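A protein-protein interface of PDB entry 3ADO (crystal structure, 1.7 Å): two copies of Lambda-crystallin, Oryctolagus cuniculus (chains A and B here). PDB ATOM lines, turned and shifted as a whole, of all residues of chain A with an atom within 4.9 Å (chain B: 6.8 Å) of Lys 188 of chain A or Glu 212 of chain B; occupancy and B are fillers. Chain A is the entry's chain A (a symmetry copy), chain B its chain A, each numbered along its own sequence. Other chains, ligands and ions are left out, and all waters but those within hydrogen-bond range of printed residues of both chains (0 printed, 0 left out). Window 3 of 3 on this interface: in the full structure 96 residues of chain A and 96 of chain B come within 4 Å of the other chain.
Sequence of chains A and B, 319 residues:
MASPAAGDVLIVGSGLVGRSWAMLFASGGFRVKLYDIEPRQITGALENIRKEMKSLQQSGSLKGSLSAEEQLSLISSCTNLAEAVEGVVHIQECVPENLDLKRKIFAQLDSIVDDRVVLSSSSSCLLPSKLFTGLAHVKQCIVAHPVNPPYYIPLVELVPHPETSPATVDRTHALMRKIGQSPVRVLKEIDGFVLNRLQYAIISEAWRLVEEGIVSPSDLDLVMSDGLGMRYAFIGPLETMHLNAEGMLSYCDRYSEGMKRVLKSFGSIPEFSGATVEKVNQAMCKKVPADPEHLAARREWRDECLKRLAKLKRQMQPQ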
ATOM      1  N   VAL A 159      26.228   0.953   3.382  1.00  0.00           N
ATOM      2  CA  VAL A 159      27.167   1.211   4.466  1.00  0.00           C
ATOM      3  C   VAL A 159      28.289   0.191   4.381  1.00  0.00           C
ATOM      4  O   VAL A 159      28.062  -1.014   4.494  1.00  0.00           O
ATOM      5  CB  VAL A 159      26.476   1.095   5.836  1.00  0.00           C
ATOM      6  CG1 VAL A 159      27.368   1.702   6.911  1.00  0.00           C
ATOM      7  CG2 VAL A 159      25.120   1.800   5.797  1.00  0.00           C
ATOM      8  N   VAL A 186      26.890   5.814   2.252  1.00  0.00           N
ATOM      9  CA  VAL A 186      27.177   6.249   3.613  1.00  0.00           C
ATOM     10  C   VAL A 186      28.681   5.972   3.662  1.00  0.00           C
ATOM     11  O   VAL A 186      29.113   4.823   3.701  1.00  0.00           O
ATOM     12  CB  VAL A 186      26.414   5.410   4.659  1.00  0.00           C
ATOM     13  CG1 VAL A 186      26.680   5.946   6.046  1.00  0.00           C
ATOM     14  CG2 VAL A 186      24.926   5.454   4.367  1.00  0.00           C
ATOM     15  N   LEU A 187      29.465   7.041   3.620  1.00  0.00           N
ATOM     16  CA  LEU A 187      30.922   6.957   3.568  1.00  0.00           C
ATOM     17  C   LEU A 187      31.638   6.260   4.714  1.00  0.00           C
ATOM     18  O   LEU A 187      32.684   5.646   4.512  1.00  0.00           O
ATOM     19  CB  LEU A 187      31.489   8.367   3.387  1.00  0.00           C
ATOM     20  CG  LEU A 187      30.840   9.103   2.212  1.00  0.00           C
ATOM     21  CD1 LEU A 187      31.361  10.527   2.136  1.00  0.00           C
ATOM     22  CD2 LEU A 187      31.121   8.345   0.924  1.00  0.00           C
ATOM     23  N   LYS A 188      31.079   6.365   5.909  1.00  0.00           N
ATOM     24  CA  LYS A 188      31.661   5.747   7.092  1.00  0.00           C
ATOM     25  C   LYS A 188      30.505   5.233   7.931  1.00  0.00           C
ATOM     26  O   LYS A 188      29.478   5.905   8.049  1.00  0.00           O
ATOM     27  CB  LYS A 188      32.457   6.778   7.896  1.00  0.00           C
ATOM     28  CG  LYS A 188      33.640   7.375   7.142  1.00  0.00           C
ATOM     29  CD  LYS A 188      34.415   8.373   7.997  1.00  0.00           C
ATOM     30  CE  LYS A 188      33.579   9.596   8.337  1.00  0.00           C
ATOM     31  NZ  LYS A 188      34.357  10.603   9.116  1.00  0.00           N
ATOM     32  N   GLU A 189      30.656   4.047   8.509  1.00  0.00           N
ATOM     33  CA  GLU A 189      29.583   3.508   9.325  1.00  0.00           C
ATOM     34  C   GLU A 189      29.340   4.405  10.529  1.00  0.00           C
ATOM     35  O   GLU A 189      30.263   5.039  11.052  1.00  0.00           O
ATOM     36  CB  GLU A 189      29.909   2.090   9.793  1.00  0.00           C
ATOM     37  CG  GLU A 189      31.149   1.984  10.663  1.00  0.00           C
ATOM     38  CD  GLU A 189      31.315   0.599  11.238  1.00  0.00           C
ATOM     39  OE1 GLU A 189      31.001  -0.371  10.518  1.00  0.00           O
ATOM     40  OE2 GLU A 189      31.764   0.479  12.400  1.00  0.00           O
ATOM     41  N   ILE A 190      28.086   4.457  10.956  1.00  0.00           N
ATOM     42  CA  ILE A 190      27.692   5.262  12.099  1.00  0.00           C
ATOM     43  C   ILE A 190      26.364   4.735  12.622  1.00  0.00           C
ATOM     44  O   ILE A 190      25.520   4.258  11.858  1.00  0.00           O
ATOM     45  CB  ILE A 190      27.572   6.765  11.718  1.00  0.00           C
ATOM     46  CG1 ILE A 190      27.419   7.615  12.981  1.00  0.00           C
ATOM     47  CG2 ILE A 190      26.387   6.979  10.784  1.00  0.00           C
ATOM     48  CD1 ILE A 190      27.489   9.119  12.720  1.00  0.00           C
ATOM     49  N   TRP B 207      23.485  18.895   8.716  1.00  0.00           N
ATOM     50  CA  TRP B 207      24.696  19.697   8.569  1.00  0.00           C
ATOM     51  C   TRP B 207      25.911  18.972   9.138  1.00  0.00           C
ATOM     52  O   TRP B 207      26.965  18.918   8.504  1.00  0.00           O
ATOM     53  CB  TRP B 207      24.511  21.040   9.272  1.00  0.00           C
ATOM     54  CG  TRP B 207      25.377  22.133   8.735  1.00  0.00           C
ATOM     55  CD1 TRP B 207      26.577  22.560   9.237  1.00  0.00           C
ATOM     56  CD2 TRP B 207      25.106  22.949   7.590  1.00  0.00           C
ATOM     57  NE1 TRP B 207      27.065  23.596   8.474  1.00  0.00           N
ATOM     58  CE2 TRP B 207      26.184  23.855   7.457  1.00  0.00           C
ATOM     59  CE3 TRP B 207      24.056  23.004   6.663  1.00  0.00           C
ATOM     60  CZ2 TRP B 207      26.241  24.806   6.432  1.00  0.00           C
ATOM     61  CZ3 TRP B 207      24.112  23.951   5.642  1.00  0.00           C
ATOM     62  CH2 TRP B 207      25.201  24.840   5.538  1.00  0.00           C
ATOM     63  N   ARG B 208      25.761  18.404  10.330  1.00  0.00           N
ATOM     64  CA  ARG B 208      26.868  17.695  10.961  1.00  0.00           C
ATOM     65  C   ARG B 208      27.254  16.413  10.227  1.00  0.00           C
ATOM     66  O   ARG B 208      28.429  16.046  10.185  1.00  0.00           O
ATOM     67  CB  ARG B 208      26.537  17.376  12.420  1.00  0.00           C
ATOM     68  CG  ARG B 208      26.553  18.589  13.353  1.00  0.00           C
ATOM     69  CD  ARG B 208      26.446  18.155  14.810  1.00  0.00           C
ATOM     70  NE  ARG B 208      25.175  17.496  15.102  1.00  0.00           N
ATOM     71  CZ  ARG B 208      24.050  18.133  15.414  1.00  0.00           C
ATOM     72  NH1 ARG B 208      24.029  19.459  15.490  1.00  0.00           N
ATOM     73  NH2 ARG B 208      22.937  17.444  15.635  1.00  0.00           N
ATOM     74  N   LEU B 209      26.270  15.725   9.654  1.00  0.00           N
ATOM     75  CA  LEU B 209      26.557  14.493   8.929  1.00  0.00           C
ATOM     76  C   LEU B 209      27.402  14.802   7.700  1.00  0.00           C
ATOM     77  O   LEU B 209      28.261  14.010   7.311  1.00  0.00           O
ATOM     78  CB  LEU B 209      25.260  13.795   8.516  1.00  0.00           C
ATOM     79  CG  LEU B 209      24.453  13.193   9.670  1.00  0.00           C
ATOM     80  CD1 LEU B 209      23.122  12.666   9.158  1.00  0.00           C
ATOM     81  CD2 LEU B 209      25.259  12.070  10.321  1.00  0.00           C
ATOM     82  N   VAL B 210      27.156  15.952   7.085  1.00  0.00           N
ATOM     83  CA  VAL B 210      27.930  16.344   5.912  1.00  0.00           C
ATOM     84  C   VAL B 210      29.315  16.791   6.380  1.00  0.00           C
ATOM     85  O   VAL B 210      30.334  16.413   5.797  1.00  0.00           O
ATOM     86  CB  VAL B 210      27.254  17.505   5.149  1.00  0.00           C
ATOM     87  CG1 VAL B 210      28.176  18.008   4.044  1.00  0.00           C
ATOM     88  CG2 VAL B 210      25.930  17.036   4.554  1.00  0.00           C
ATOM     89  N   GLU B 211      29.342  17.586   7.443  1.00  0.00           N
ATOM     90  CA  GLU B 211      30.598  18.084   7.991  1.00  0.00           C
ATOM     91  C   GLU B 211      31.521  16.935   8.402  1.00  0.00           C
ATOM     92  O   GLU B 211      32.727  16.976   8.149  1.00  0.00           O
ATOM     93  CB  GLU B 211      30.318  18.979   9.200  1.00  0.00           C
ATOM     94  CG  GLU B 211      31.560  19.574   9.842  1.00  0.00           C
ATOM     95  CD  GLU B 211      31.226  20.521  10.978  1.00  0.00           C
ATOM     96  OE1 GLU B 211      30.580  20.082  11.952  1.00  0.00           O
ATOM     97  OE2 GLU B 211      31.611  21.705  10.898  1.00  0.00           O
ATOM     98  N   GLU B 212      30.945  15.909   9.023  1.00  0.00           N
ATOM     99  CA  GLU B 212      31.708  14.751   9.483  1.00  0.00           C
ATOM    100  C   GLU B 212      32.074  13.747   8.394  1.00  0.00           C
ATOM    101  O   GLU B 212      32.723  12.738   8.671  1.00  0.00           O
ATOM    102  CB  GLU B 212      30.946  14.031  10.597  1.00  0.00           C
ATOM    103  CG  GLU B 212      30.851  14.820  11.893  1.00  0.00           C
ATOM    104  CD  GLU B 212      32.215  15.174  12.454  1.00  0.00           C
ATOM    105  OE1 GLU B 212      33.032  14.247  12.657  1.00  0.00           O
ATOM    106  OE2 GLU B 212      32.472  16.374  12.694  1.00  0.00           O
ATOM    107  N   GLY B 213      31.654  14.017   7.162  1.00  0.00           N
ATOM    108  CA  GLY B 213      31.967  13.129   6.057  1.00  0.00           C
ATOM    109  C   GLY B 213      31.238  11.797   6.080  1.00  0.00           C
ATOM    110  O   GLY B 213      31.772  10.775   5.638  1.00  0.00           O
ATOM    111  N   ILE B 214      30.018  11.799   6.598  1.00  0.00           N
ATOM    112  CA  ILE B 214      29.229  10.578   6.663  1.00  0.00           C
ATOM    113  C   ILE B 214      28.507  10.355   5.337  1.00  0.00           C
ATOM    114  O   ILE B 214      28.319   9.219   4.898  1.00  0.00           O
ATOM    115  CB  ILE B 214      28.181  10.655   7.790  1.00  0.00           C
ATOM    116  CG1 ILE B 214      28.875  10.907   9.129  1.00  0.00           C
ATOM    117  CG2 ILE B 214      27.363   9.371   7.830  1.00  0.00           C
ATOM    118  CD1 ILE B 214      29.886   9.845   9.519  1.00  0.00           C
ATOM    119  N   VAL B 215      28.126  11.449   4.690  1.00  0.00           N
ATOM    120  CA  VAL B 215      27.399  11.370   3.432  1.00  0.00           C
ATOM    121  C   VAL B 215      27.525  12.692   2.680  1.00  0.00           C
ATOM    122  O   VAL B 215      27.701  13.743   3.293  1.00  0.00           O
ATOM    123  CB  VAL B 215      25.907  11.055   3.704  1.00  0.00           C
ATOM    124  CG1 VAL B 215      25.263  12.203   4.469  1.00  0.00           C
ATOM    125  CG2 VAL B 215      25.181  10.786   2.412  1.00  0.00           C
ATOM    126  N   THR B 276      31.974  24.078   5.664  1.00  0.00           N
ATOM    127  CA  THR B 276      30.767  23.297   5.422  1.00  0.00           C
ATOM    128  C   THR B 276      29.715  24.015   4.587  1.00  0.00           C
ATOM    129  O   THR B 276      29.042  23.388   3.768  1.00  0.00           O
ATOM    130  CB  THR B 276      30.137  22.816   6.744  1.00  0.00           C
ATOM    131  OG1 THR B 276      31.119  22.099   7.506  1.00  0.00           O
ATOM    132  CG2 THR B 276      28.967  21.878   6.463  1.00  0.00           C
ATOM    133  N   LYS B 279      30.930  23.746   1.161  1.00  0.00           N
ATOM    134  CA  LYS B 279      30.779  22.383   0.673  1.00  0.00           C
ATOM    135  C   LYS B 279      29.324  22.120   0.308  1.00  0.00           C
ATOM    136  O   LYS B 279      29.026  21.571  -0.753  1.00  0.00           O
ATOM    137  CB  LYS B 279      31.228  21.387   1.740  1.00  0.00           C
ATOM    138  CG  LYS B 279      31.130  19.939   1.308  1.00  0.00           C
ATOM    139  CD  LYS B 279      31.821  19.034   2.312  1.00  0.00           C
ATOM    140  CE  LYS B 279      31.973  17.624   1.767  1.00  0.00           C
ATOM    141  NZ  LYS B 279      32.869  16.805   2.629  1.00  0.00           N
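The backbone carbonyl oxygen (O) of Glu 212 of chain B is in hydrogen-bond range of the side-chain amino group (NZ) of Lys 188 of chain A (2.7 Å).
The backbone carbonyl oxygen of Ile 214 of chain B lies within hydrogen-bond range of the backbone NH of Leu 187 of chain A.
The backbone carbonyl oxygen (O) of Leu 209 of chain B sits at hydrogen-bond distance from the backbone NH (N) of Ile 214 of chain B, 2.9 Å away.
Among the printed residues, merely in contact across the chains: Leu 187 of chain A with Gly 213 of chain B (3.3 Å), Val 186 of chain A with Ile 214 of chain B (3.4 Å), Lys 188 of chain A with Gly 213 of chain B (3.5 Å), Lys 188 of chain A with Ile 214 of chain B (3.9 Å) and Ile 190 of chain A with Ile 214 of chain B (3.9 Å).
Of the printed residues of chain B, Val 186 of chain A touches Ile 214.
Of chain B, only Glu 212 (2.7 Å), Gly 213 (3.5 Å) and Ile 214 (3.9 Å) come within 4 Å of Lys 188 of chain A.
Trp 207 of chain B touches none of the printed residues of chain A.
Glu 211 of chain B touches none of the printed residues of chain A.
Of the printed residues of chain A, Glu 212 of chain B touches Lys 188.
Printed residues of chain A within 4 Å of Gly 213 of chain B: Leu 187 (3.3 Å) and Lys 188 (3.5 Å).
The nearest residue of chain B that does not touch Lys 188 of chain A is Val 215 of chain B (6.0 Å).
Of the 6 printed residues of chain A, 4 touch a printed residue of chain B.
Printed residues of chain A that touch a printed residue of chain B: Val 186, Leu 187, Lys 188 and Ile 190.
Hydrophobic or aromatic side chains of chain A that line the printed part of chain B: Val 186, Leu 187 and Ile 190.
Among the printed residues, 7 pairs touch across the chains.
Among the printed residues, no Asp or Glu carboxylate lies within 4 Å of a Lys or Arg side-chain nitrogen of the other chain.
No position is printed for both chains.
Of the 7 pairs that touch across the chains among the printed residues, none has its exchanged pair printed and touching as well.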
